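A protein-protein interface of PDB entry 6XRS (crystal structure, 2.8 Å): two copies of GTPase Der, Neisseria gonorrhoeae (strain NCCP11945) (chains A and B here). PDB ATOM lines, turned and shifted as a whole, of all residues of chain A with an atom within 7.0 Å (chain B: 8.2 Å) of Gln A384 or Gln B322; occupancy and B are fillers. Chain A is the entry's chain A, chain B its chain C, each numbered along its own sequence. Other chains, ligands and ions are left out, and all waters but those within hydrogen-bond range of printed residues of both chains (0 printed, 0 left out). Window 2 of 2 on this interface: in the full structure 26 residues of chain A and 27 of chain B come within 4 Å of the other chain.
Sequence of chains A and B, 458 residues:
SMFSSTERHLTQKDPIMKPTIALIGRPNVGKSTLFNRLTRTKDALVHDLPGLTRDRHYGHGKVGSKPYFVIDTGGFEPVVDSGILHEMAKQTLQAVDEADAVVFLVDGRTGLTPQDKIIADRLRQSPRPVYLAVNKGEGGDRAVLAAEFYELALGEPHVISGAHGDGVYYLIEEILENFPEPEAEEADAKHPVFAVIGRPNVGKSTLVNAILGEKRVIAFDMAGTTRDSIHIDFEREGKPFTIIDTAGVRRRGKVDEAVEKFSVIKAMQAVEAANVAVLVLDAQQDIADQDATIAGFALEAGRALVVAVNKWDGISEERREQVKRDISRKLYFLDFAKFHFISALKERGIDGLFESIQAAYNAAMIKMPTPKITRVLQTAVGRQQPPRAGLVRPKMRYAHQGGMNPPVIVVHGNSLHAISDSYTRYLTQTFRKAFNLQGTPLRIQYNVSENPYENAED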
ATOM      1  N   THR A 379      -2.546  22.459  13.817  1.00  0.00           N
ATOM      2  CA  THR A 379      -2.649  22.454  12.367  1.00  0.00           C
ATOM      3  C   THR A 379      -1.276  22.491  11.725  1.00  0.00           C
ATOM      4  O   THR A 379      -0.988  21.700  10.819  1.00  0.00           O
ATOM      5  CB  THR A 379      -3.532  23.596  11.890  1.00  0.00           C
ATOM      6  OG1 THR A 379      -4.871  23.347  12.348  1.00  0.00           O
ATOM      7  CG2 THR A 379      -3.514  23.658  10.377  1.00  0.00           C
ATOM      8  N   ALA A 380      -0.406  23.372  12.213  1.00  0.00           N
ATOM      9  CA  ALA A 380       0.951  23.435  11.690  1.00  0.00           C
ATOM     10  C   ALA A 380       1.639  22.079  11.784  1.00  0.00           C
ATOM     11  O   ALA A 380       2.285  21.637  10.828  1.00  0.00           O
ATOM     12  CB  ALA A 380       1.750  24.482  12.466  1.00  0.00           C
ATOM     13  N   VAL A 381       1.493  21.399  12.924  1.00  0.00           N
ATOM     14  CA  VAL A 381       2.141  20.109  13.130  1.00  0.00           C
ATOM     15  C   VAL A 381       1.520  19.047  12.234  1.00  0.00           C
ATOM     16  O   VAL A 381       2.211  18.141  11.752  1.00  0.00           O
ATOM     17  CB  VAL A 381       2.072  19.718  14.616  1.00  0.00           C
ATOM     18  CG1 VAL A 381       2.535  18.296  14.820  1.00  0.00           C
ATOM     19  CG2 VAL A 381       2.885  20.683  15.460  1.00  0.00           C
ATOM     20  N   GLY A 382       0.207  19.121  12.014  1.00  0.00           N
ATOM     21  CA  GLY A 382      -0.432  18.150  11.141  1.00  0.00           C
ATOM     22  C   GLY A 382       0.029  18.270   9.703  1.00  0.00           C
ATOM     23  O   GLY A 382       0.163  17.266   8.999  1.00  0.00           O
ATOM     24  N   ARG A 383       0.303  19.495   9.253  1.00  0.00           N
ATOM     25  CA  ARG A 383       0.729  19.699   7.875  1.00  0.00           C
ATOM     26  C   ARG A 383       2.195  19.328   7.680  1.00  0.00           C
ATOM     27  O   ARG A 383       2.564  18.759   6.646  1.00  0.00           O
ATOM     28  CB  ARG A 383       0.478  21.155   7.467  1.00  0.00           C
ATOM     29  N   GLN A 384       3.033  19.587   8.679  1.00  0.00           N
ATOM     30  CA  GLN A 384       4.452  19.258   8.614  1.00  0.00           C
ATOM     31  C   GLN A 384       4.885  18.803   9.999  1.00  0.00           C
ATOM     32  O   GLN A 384       5.016  19.614  10.921  1.00  0.00           O
ATOM     33  CB  GLN A 384       5.270  20.456   8.126  1.00  0.00           C
ATOM     34  CG  GLN A 384       6.754  20.188   7.867  1.00  0.00           C
ATOM     35  CD  GLN A 384       7.528  21.474   7.557  1.00  0.00           C
ATOM     36  OE1 GLN A 384       6.962  22.442   7.028  1.00  0.00           O
ATOM     37  NE2 GLN A 384       8.825  21.486   7.878  1.00  0.00           N
ATOM     38  N   GLN A 385       5.103  17.503  10.136  1.00  0.00           N
ATOM     39  CA  GLN A 385       5.516  16.935  11.403  1.00  0.00           C
ATOM     40  C   GLN A 385       6.929  17.408  11.736  1.00  0.00           C
ATOM     41  O   GLN A 385       7.695  17.786  10.844  1.00  0.00           O
ATOM     42  CB  GLN A 385       5.476  15.406  11.340  1.00  0.00           C
ATOM     43  CG  GLN A 385       4.086  14.799  11.223  1.00  0.00           C
ATOM     44  CD  GLN A 385       3.293  14.885  12.525  1.00  0.00           C
ATOM     45  OE1 GLN A 385       3.846  15.198  13.584  1.00  0.00           O
ATOM     46  NE2 GLN A 385       1.988  14.604  12.448  1.00  0.00           N
ATOM     47  N   PRO A 386       7.288  17.444  13.015  1.00  0.00           N
ATOM     48  CA  PRO A 386       8.675  17.719  13.359  1.00  0.00           C
ATOM     49  C   PRO A 386       9.567  16.633  12.786  1.00  0.00           C
ATOM     50  O   PRO A 386       9.111  15.503  12.530  1.00  0.00           O
ATOM     51  CB  PRO A 386       8.671  17.713  14.894  1.00  0.00           C
ATOM     52  CG  PRO A 386       7.237  17.853  15.286  1.00  0.00           C
ATOM     53  CD  PRO A 386       6.462  17.187  14.206  1.00  0.00           C
ATOM     54  N   PRO A 387      10.838  16.949  12.517  1.00  0.00           N
ATOM     55  CA  PRO A 387      11.733  16.017  11.815  1.00  0.00           C
ATOM     56  C   PRO A 387      12.062  14.705  12.549  1.00  0.00           C
ATOM     57  O   PRO A 387      12.644  14.686  13.633  1.00  0.00           O
ATOM     58  CB  PRO A 387      12.999  16.863  11.623  1.00  0.00           C
ATOM     59  CG  PRO A 387      12.927  17.901  12.726  1.00  0.00           C
ATOM     60  CD  PRO A 387      11.484  18.243  12.795  1.00  0.00           C
ATOM     61  N   SER A 420      14.912  21.397  16.133  1.00  0.00           N
ATOM     62  CA  SER A 420      15.825  22.129  15.276  1.00  0.00           C
ATOM     63  C   SER A 420      15.458  23.604  15.226  1.00  0.00           C
ATOM     64  O   SER A 420      14.300  23.986  15.409  1.00  0.00           O
ATOM     65  CB  SER A 420      15.813  21.516  13.874  1.00  0.00           C
ATOM     66  OG  SER A 420      14.548  21.660  13.256  1.00  0.00           O
ATOM     67  N   ASP A 421      16.469  24.444  15.003  1.00  0.00           N
ATOM     68  CA  ASP A 421      16.197  25.867  14.879  1.00  0.00           C
ATOM     69  C   ASP A 421      15.322  26.133  13.661  1.00  0.00           C
ATOM     70  O   ASP A 421      14.507  27.065  13.667  1.00  0.00           O
ATOM     71  CB  ASP A 421      17.504  26.661  14.811  1.00  0.00           C
ATOM     72  CG  ASP A 421      17.292  28.106  14.348  1.00  0.00           C
ATOM     73  OD1 ASP A 421      16.686  28.902  15.116  1.00  0.00           O
ATOM     74  OD2 ASP A 421      17.722  28.452  13.217  1.00  0.00           O
ATOM     75  N   SER A 422      15.468  25.319  12.612  1.00  0.00           N
ATOM     76  CA  SER A 422      14.702  25.537  11.390  1.00  0.00           C
ATOM     77  C   SER A 422      13.227  25.201  11.566  1.00  0.00           C
ATOM     78  O   SER A 422      12.373  25.850  10.946  1.00  0.00           O
ATOM     79  CB  SER A 422      15.283  24.714  10.243  1.00  0.00           C
ATOM     80  OG  SER A 422      15.226  23.333  10.539  1.00  0.00           O
ATOM     81  N   TYR A 423      12.894  24.202  12.393  1.00  0.00           N
ATOM     82  CA  TYR A 423      11.479  23.925  12.612  1.00  0.00           C
ATOM     83  C   TYR A 423      10.844  25.027  13.450  1.00  0.00           C
ATOM     84  O   TYR A 423       9.767  25.528  13.110  1.00  0.00           O
ATOM     85  CB  TYR A 423      11.290  22.572  13.286  1.00  0.00           C
ATOM     86  CG  TYR A 423       9.869  22.038  13.180  1.00  0.00           C
ATOM     87  CD1 TYR A 423       9.420  21.446  12.011  1.00  0.00           C
ATOM     88  CD2 TYR A 423       8.972  22.150  14.230  1.00  0.00           C
ATOM     89  CE1 TYR A 423       8.137  20.957  11.900  1.00  0.00           C
ATOM     90  CE2 TYR A 423       7.677  21.668  14.117  1.00  0.00           C
ATOM     91  CZ  TYR A 423       7.271  21.071  12.950  1.00  0.00           C
ATOM     92  OH  TYR A 423       5.990  20.584  12.815  1.00  0.00           O
ATOM     93  N   THR A 424      11.522  25.446  14.525  1.00  0.00           N
ATOM     94  CA  THR A 424      11.068  26.584  15.313  1.00  0.00           C
ATOM     95  C   THR A 424      10.864  27.821  14.440  1.00  0.00           C
ATOM     96  O   THR A 424      10.020  28.674  14.744  1.00  0.00           O
ATOM     97  CB  THR A 424      12.074  26.865  16.431  1.00  0.00           C
ATOM     98  OG1 THR A 424      12.220  25.699  17.238  1.00  0.00           O
ATOM     99  CG2 THR A 424      11.633  28.033  17.304  1.00  0.00           C
ATOM    100  N   ARG A 425      11.645  27.952  13.369  1.00  0.00           N
ATOM    101  CA  ARG A 425      11.431  29.052  12.443  1.00  0.00           C
ATOM    102  C   ARG A 425      10.110  28.875  11.691  1.00  0.00           C
ATOM    103  O   ARG A 425       9.348  29.839  11.524  1.00  0.00           O
ATOM    104  CB  ARG A 425      12.624  29.144  11.493  1.00  0.00           C
ATOM    105  CG  ARG A 425      12.572  30.305  10.530  1.00  0.00           C
ATOM    106  CD  ARG A 425      13.861  30.423   9.715  1.00  0.00           C
ATOM    107  NE  ARG A 425      13.777  31.538   8.775  1.00  0.00           N
ATOM    108  CZ  ARG A 425      14.106  32.789   9.078  1.00  0.00           C
ATOM    109  NH1 ARG A 425      14.564  33.071  10.294  1.00  0.00           N
ATOM    110  NH2 ARG A 425      13.983  33.755   8.169  1.00  0.00           N
ATOM    111  N   TYR A 426       9.800  27.637  11.278  1.00  0.00           N
ATOM    112  CA  TYR A 426       8.528  27.350  10.613  1.00  0.00           C
ATOM    113  C   TYR A 426       7.339  27.640  11.524  1.00  0.00           C
ATOM    114  O   TYR A 426       6.353  28.253  11.095  1.00  0.00           O
ATOM    115  CB  TYR A 426       8.529  25.894  10.123  1.00  0.00           C
ATOM    116  CG  TYR A 426       7.169  25.258   9.876  1.00  0.00           C
ATOM    117  CD1 TYR A 426       6.331  25.689   8.851  1.00  0.00           C
ATOM    118  CD2 TYR A 426       6.753  24.166  10.638  1.00  0.00           C
ATOM    119  CE1 TYR A 426       5.089  25.080   8.633  1.00  0.00           C
ATOM    120  CE2 TYR A 426       5.521  23.543  10.415  1.00  0.00           C
ATOM    121  CZ  TYR A 426       4.698  24.003   9.422  1.00  0.00           C
ATOM    122  OH  TYR A 426       3.487  23.386   9.238  1.00  0.00           O
ATOM    123  N   LEU A 427       7.426  27.235  12.795  1.00  0.00           N
ATOM    124  CA  LEU A 427       6.361  27.551  13.745  1.00  0.00           C
ATOM    125  C   LEU A 427       6.264  29.052  13.999  1.00  0.00           C
ATOM    126  O   LEU A 427       5.158  29.613  14.003  1.00  0.00           O
ATOM    127  CB  LEU A 427       6.591  26.799  15.054  1.00  0.00           C
ATOM    128  CG  LEU A 427       6.360  25.286  15.018  1.00  0.00           C
ATOM    129  CD1 LEU A 427       6.455  24.696  16.403  1.00  0.00           C
ATOM    130  CD2 LEU A 427       5.008  24.983  14.410  1.00  0.00           C
ATOM    131  N   GLN A 429       7.080  31.560  12.028  1.00  0.00           N
ATOM    132  CA  GLN A 429       6.399  32.167  10.884  1.00  0.00           C
ATOM    133  C   GLN A 429       4.920  31.791  10.858  1.00  0.00           C
ATOM    134  O   GLN A 429       4.060  32.651  10.610  1.00  0.00           O
ATOM    135  CB  GLN A 429       7.070  31.758   9.571  1.00  0.00           C
ATOM    136  CG  GLN A 429       8.314  32.553   9.236  1.00  0.00           C
ATOM    137  CD  GLN A 429       9.164  31.898   8.165  1.00  0.00           C
ATOM    138  OE1 GLN A 429       8.881  30.774   7.732  1.00  0.00           O
ATOM    139  NE2 GLN A 429      10.217  32.591   7.739  1.00  0.00           N
ATOM    140  N   ASP B 286      20.250  20.415  11.086  1.00  0.00           N
ATOM    141  CA  ASP B 286      20.619  21.815  10.942  1.00  0.00           C
ATOM    142  C   ASP B 286      22.118  21.949  10.738  1.00  0.00           C
ATOM    143  O   ASP B 286      22.909  21.141  11.231  1.00  0.00           O
ATOM    144  CB  ASP B 286      20.224  22.619  12.179  1.00  0.00           C
ATOM    145  CG  ASP B 286      18.739  22.900  12.267  1.00  0.00           C
ATOM    146  OD1 ASP B 286      17.992  22.654  11.287  1.00  0.00           O
ATOM    147  OD2 ASP B 286      18.327  23.386  13.345  1.00  0.00           O
ATOM    148  N   TRP B 312      20.099  13.713   0.622  1.00  0.00           N
ATOM    149  CA  TRP B 312      18.973  14.408   0.018  1.00  0.00           C
ATOM    150  C   TRP B 312      17.792  13.476  -0.228  1.00  0.00           C
ATOM    151  O   TRP B 312      16.657  13.955  -0.348  1.00  0.00           O
ATOM    152  CB  TRP B 312      19.436  15.056  -1.289  1.00  0.00           C
ATOM    153  CG  TRP B 312      18.559  16.158  -1.792  1.00  0.00           C
ATOM    154  CD1 TRP B 312      17.906  16.192  -2.986  1.00  0.00           C
ATOM    155  CD2 TRP B 312      18.264  17.396  -1.139  1.00  0.00           C
ATOM    156  NE1 TRP B 312      17.205  17.370  -3.117  1.00  0.00           N
ATOM    157  CE2 TRP B 312      17.405  18.126  -1.993  1.00  0.00           C
ATOM    158  CE3 TRP B 312      18.627  17.954   0.086  1.00  0.00           C
ATOM    159  CZ2 TRP B 312      16.905  19.384  -1.654  1.00  0.00           C
ATOM    160  CZ3 TRP B 312      18.131  19.207   0.420  1.00  0.00           C
ATOM    161  CH2 TRP B 312      17.279  19.908  -0.447  1.00  0.00           C
ATOM    162  N   ILE B 315      14.883  13.960   2.339  1.00  0.00           N
ATOM    163  CA  ILE B 315      14.057  15.163   2.395  1.00  0.00           C
ATOM    164  C   ILE B 315      12.827  15.020   1.496  1.00  0.00           C
ATOM    165  O   ILE B 315      12.947  14.714   0.304  1.00  0.00           O
ATOM    166  CB  ILE B 315      14.885  16.396   2.006  1.00  0.00           C
ATOM    167  CG1 ILE B 315      16.300  16.278   2.597  1.00  0.00           C
ATOM    168  CG2 ILE B 315      14.171  17.678   2.431  1.00  0.00           C
ATOM    169  CD1 ILE B 315      16.353  16.248   4.113  1.00  0.00           C
ATOM    170  N   SER B 316      11.640  15.243   2.063  1.00  0.00           N
ATOM    171  CA  SER B 316      10.444  15.390   1.245  1.00  0.00           C
ATOM    172  C   SER B 316      10.468  16.723   0.494  1.00  0.00           C
ATOM    173  O   SER B 316      11.208  17.646   0.840  1.00  0.00           O
ATOM    174  CB  SER B 316       9.186  15.335   2.101  1.00  0.00           C
ATOM    175  OG  SER B 316       9.068  16.520   2.871  1.00  0.00           O
ATOM    176  N   GLU B 317       9.617  16.831  -0.533  1.00  0.00           N
ATOM    177  CA  GLU B 317       9.655  18.012  -1.391  1.00  0.00           C
ATOM    178  C   GLU B 317       9.291  19.282  -0.634  1.00  0.00           C
ATOM    179  O   GLU B 317       9.953  20.315  -0.800  1.00  0.00           O
ATOM    180  CB  GLU B 317       8.734  17.844  -2.598  1.00  0.00           C
ATOM    181  CG  GLU B 317       9.212  18.621  -3.827  1.00  0.00           C
ATOM    182  CD  GLU B 317      10.580  18.172  -4.308  1.00  0.00           C
ATOM    183  OE1 GLU B 317      10.762  16.945  -4.466  1.00  0.00           O
ATOM    184  OE2 GLU B 317      11.475  19.029  -4.517  1.00  0.00           O
ATOM    185  N   GLU B 318       8.232  19.238   0.184  1.00  0.00           N
ATOM    186  CA  GLU B 318       7.846  20.412   0.969  1.00  0.00           C
ATOM    187  C   GLU B 318       9.045  20.969   1.734  1.00  0.00           C
ATOM    188  O   GLU B 318       9.314  22.179   1.714  1.00  0.00           O
ATOM    189  CB  GLU B 318       6.700  20.056   1.923  1.00  0.00           C
ATOM    190  N   ARG B 319       9.800  20.085   2.388  1.00  0.00           N
ATOM    191  CA  ARG B 319      10.962  20.485   3.169  1.00  0.00           C
ATOM    192  C   ARG B 319      12.146  20.920   2.319  1.00  0.00           C
ATOM    193  O   ARG B 319      13.103  21.472   2.872  1.00  0.00           O
ATOM    194  CB  ARG B 319      11.417  19.329   4.059  1.00  0.00           C
ATOM    195  CG  ARG B 319      10.411  18.837   5.077  1.00  0.00           C
ATOM    196  CD  ARG B 319      11.161  18.063   6.132  1.00  0.00           C
ATOM    197  NE  ARG B 319      12.289  18.863   6.595  1.00  0.00           N
ATOM    198  CZ  ARG B 319      13.438  18.359   7.023  1.00  0.00           C
ATOM    199  NH1 ARG B 319      13.619  17.044   7.050  1.00  0.00           N
ATOM    200  NH2 ARG B 319      14.410  19.174   7.418  1.00  0.00           N
ATOM    201  N   ARG B 320      12.110  20.710   1.001  1.00  0.00           N
ATOM    202  CA  ARG B 320      13.335  20.867   0.222  1.00  0.00           C
ATOM    203  C   ARG B 320      13.740  22.329   0.098  1.00  0.00           C
ATOM    204  O   ARG B 320      14.916  22.663   0.295  1.00  0.00           O
ATOM    205  CB  ARG B 320      13.177  20.203  -1.145  1.00  0.00           C
ATOM    206  CG  ARG B 320      13.651  18.757  -1.078  1.00  0.00           C
ATOM    207  CD  ARG B 320      13.661  17.999  -2.399  1.00  0.00           C
ATOM    208  NE  ARG B 320      14.262  16.677  -2.206  1.00  0.00           N
ATOM    209  CZ  ARG B 320      14.420  15.772  -3.164  1.00  0.00           C
ATOM    210  NH1 ARG B 320      14.006  16.036  -4.393  1.00  0.00           N
ATOM    211  NH2 ARG B 320      14.999  14.610  -2.892  1.00  0.00           N
ATOM    212  N   GLU B 321      12.784  23.220  -0.181  1.00  0.00           N
ATOM    213  CA  GLU B 321      13.123  24.637  -0.250  1.00  0.00           C
ATOM    214  C   GLU B 321      13.467  25.191   1.122  1.00  0.00           C
ATOM    215  O   GLU B 321      14.407  25.981   1.258  1.00  0.00           O
ATOM    216  CB  GLU B 321      11.979  25.424  -0.877  1.00  0.00           C
ATOM    217  CG  GLU B 321      11.941  25.271  -2.368  1.00  0.00           C
ATOM    218  CD  GLU B 321      13.338  25.234  -2.948  1.00  0.00           C
ATOM    219  OE1 GLU B 321      13.663  24.227  -3.614  1.00  0.00           O
ATOM    220  OE2 GLU B 321      14.128  26.181  -2.690  1.00  0.00           O
ATOM    221  N   GLN B 322      12.741  24.760   2.152  1.00  0.00           N
ATOM    222  CA  GLN B 322      13.071  25.163   3.512  1.00  0.00           C
ATOM    223  C   GLN B 322      14.507  24.807   3.880  1.00  0.00           C
ATOM    224  O   GLN B 322      15.144  25.533   4.651  1.00  0.00           O
ATOM    225  CB  GLN B 322      12.079  24.519   4.480  1.00  0.00           C
ATOM    226  CG  GLN B 322      12.490  24.522   5.937  1.00  0.00           C
ATOM    227  CD  GLN B 322      11.361  24.093   6.871  1.00  0.00           C
ATOM    228  OE1 GLN B 322      10.419  23.393   6.471  1.00  0.00           O
ATOM    229  NE2 GLN B 322      11.446  24.530   8.125  1.00  0.00           N
ATOM    230  N   VAL B 323      15.062  23.753   3.290  1.00  0.00           N
ATOM    231  CA  VAL B 323      16.416  23.330   3.642  1.00  0.00           C
ATOM    232  C   VAL B 323      17.447  24.036   2.772  1.00  0.00           C
ATOM    233  O   VAL B 323      18.527  24.391   3.249  1.00  0.00           O
ATOM    234  CB  VAL B 323      16.548  21.795   3.549  1.00  0.00           C
ATOM    235  CG1 VAL B 323      17.971  21.370   3.805  1.00  0.00           C
ATOM    236  CG2 VAL B 323      15.639  21.113   4.535  1.00  0.00           C
ATOM    237  N   LYS B 324      17.149  24.210   1.480  1.00  0.00           N
ATOM    238  CA  LYS B 324      17.990  25.054   0.637  1.00  0.00           C
ATOM    239  C   LYS B 324      18.042  26.482   1.174  1.00  0.00           C
ATOM    240  O   LYS B 324      19.115  27.079   1.260  1.00  0.00           O
ATOM    241  CB  LYS B 324      17.484  25.036  -0.804  1.00  0.00           C
ATOM    242  CG  LYS B 324      17.914  23.831  -1.602  1.00  0.00           C
ATOM    243  CD  LYS B 324      17.378  23.845  -3.038  1.00  0.00           C
ATOM    244  CE  LYS B 324      17.929  22.644  -3.827  1.00  0.00           C
ATOM    245  NZ  LYS B 324      17.412  22.551  -5.235  1.00  0.00           N
ATOM    246  N   ARG B 325      16.898  27.044   1.559  1.00  0.00           N
ATOM    247  CA  ARG B 325      16.922  28.390   2.123  1.00  0.00           C
ATOM    248  C   ARG B 325      17.732  28.417   3.414  1.00  0.00           C
ATOM    249  O   ARG B 325      18.552  29.317   3.619  1.00  0.00           O
ATOM    250  CB  ARG B 325      15.492  28.902   2.346  1.00  0.00           C
ATOM    251  CG  ARG B 325      15.239  30.333   1.844  1.00  0.00           C
ATOM    252  CD  ARG B 325      13.764  30.568   1.456  1.00  0.00           C
ATOM    253  NE  ARG B 325      12.826  29.858   2.335  1.00  0.00           N
ATOM    254  CZ  ARG B 325      12.029  28.858   1.952  1.00  0.00           C
ATOM    255  NH1 ARG B 325      12.032  28.445   0.684  1.00  0.00           N
ATOM    256  NH2 ARG B 325      11.223  28.271   2.834  1.00  0.00           N
ATOM    257  N   ASP B 326      17.548  27.408   4.274  1.00  0.00           N
ATOM    258  CA  ASP B 326      18.307  27.322   5.520  1.00  0.00           C
ATOM    259  C   ASP B 326      19.808  27.240   5.257  1.00  0.00           C
ATOM    260  O   ASP B 326      20.608  27.897   5.929  1.00  0.00           O
ATOM    261  CB  ASP B 326      17.857  26.084   6.299  1.00  0.00           C
ATOM    262  CG  ASP B 326      18.261  26.113   7.782  1.00  0.00           C
ATOM    263  OD1 ASP B 326      17.538  26.792   8.565  1.00  0.00           O
ATOM    264  OD2 ASP B 326      19.288  25.461   8.151  1.00  0.00           O
ATOM    265  N   ILE B 327      20.213  26.476   4.252  1.00  0.00           N
ATOM    266  CA  ILE B 327      21.639  26.237   4.071  1.00  0.00           C
ATOM    267  C   ILE B 327      22.323  27.468   3.499  1.00  0.00           C
ATOM    268  O   ILE B 327      23.457  27.788   3.871  1.00  0.00           O
ATOM    269  CB  ILE B 327      21.872  24.986   3.205  1.00  0.00           C
ATOM    270  CG1 ILE B 327      21.647  23.716   4.027  1.00  0.00           C
ATOM    271  CG2 ILE B 327      23.271  24.977   2.645  1.00  0.00           C
ATOM    272  CD1 ILE B 327      21.667  22.441   3.213  1.00  0.00           C
ATOM    273  N   SER B 328      21.676  28.164   2.562  1.00  0.00           N
ATOM    274  CA  SER B 328      22.297  29.379   2.037  1.00  0.00           C
ATOM    275  C   SER B 328      22.304  30.484   3.086  1.00  0.00           C
ATOM    276  O   SER B 328      23.251  31.273   3.150  1.00  0.00           O
ATOM    277  CB  SER B 328      21.589  29.837   0.761  1.00  0.00           C
ATOM    278  OG  SER B 328      20.296  30.334   1.055  1.00  0.00           O
ATOM    279  N   ARG B 329      21.307  30.505   3.965  1.00  0.00           N
ATOM    280  CA  ARG B 329      21.286  31.499   5.028  1.00  0.00           C
ATOM    281  C   ARG B 329      22.434  31.272   6.003  1.00  0.00           C
ATOM    282  O   ARG B 329      23.037  32.232   6.487  1.00  0.00           O
ATOM    283  CB  ARG B 329      19.922  31.465   5.734  1.00  0.00           C
ATOM    284  CG  ARG B 329      19.764  32.298   6.999  1.00  0.00           C
ATOM    285  CD  ARG B 329      18.307  32.183   7.573  1.00  0.00           C
ATOM    286  NE  ARG B 329      17.903  30.803   7.897  1.00  0.00           N
ATOM    287  CZ  ARG B 329      18.007  30.207   9.092  1.00  0.00           C
ATOM    288  NH1 ARG B 329      18.494  30.879  10.139  1.00  0.00           N
ATOM    289  NH2 ARG B 329      17.610  28.935   9.239  1.00  0.00           N
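The side-chain amide oxygen (OE1) of Gln B322 lies within hydrogen-bond range of the side-chain amide nitrogen (NE2) of Gln A384. The backbone NH (N) of Asp A421 is in hydrogen-bond range of the side-chain carboxylate (OD2) of Asp B286 (2.7 Å). The guanidinium group (NH1) of Arg B329 is in salt-bridge range of the side-chain carboxylate (OD2) of Asp A421 (3.995 Å). OG of Ser A422 is in hydrogen-bond range of OD1 of Asp B286, at 2.9 Å. O of Ser A422 lies within hydrogen-bond range of NE2 of Gln B322 (3.2 Å).
O of Ala A380 sits at hydrogen-bond distance from OH of Tyr A426 (2.7 Å). OG of Ser A422 sits at hydrogen-bond distance from OG of Ser A420. The backbone NH (N) of Tyr A423 sits at hydrogen-bond distance from the side-chain hydroxyl (OG) of Ser A420. The backbone carbonyl oxygen (O) of Ser A420 lies within hydrogen-bond range of the side-chain hydroxyl (OG1) of Thr A424.
Ser A420 touches Asp B286. Ser A422 touches Asp B326. Tyr A426 touches Gln B322 (CB to NE2, 3.8 Å).
Gln A384 touches just one residue of chain B: Gln B322 (2.9 Å). Of the printed residues of chain B, Asp A421 touches Asp B286 (2.7 Å) and Arg B329 (3.995 Å). Printed residues of chain A within 4 Å of Asp B286: Ser A420, Asp A421 and Ser A422. Ile B315 touches none of the printed residues of chain A. Gln B322 touches three residues of chain A. Of the printed residues of chain A, Asp B326 touches Ser A422. The nearest residue of chain B that does not touch Gln A384 is Arg B319 (4.2 Å). The nearest residue of chain A that does not touch Gln B322 is Tyr A423 (4.5 Å).
Of the 18 printed residues of chain A, 5 touch a printed residue of chain B. Hydrophobic or aromatic side chains of chain A within 4 Å of the printed part of chain B: Tyr A426. Along chain A the printed residues that touch a printed residue of chain B span positions 384 to 426. Among the printed residues, 8 pairs touch across the chains.
No position is printed for both chains.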
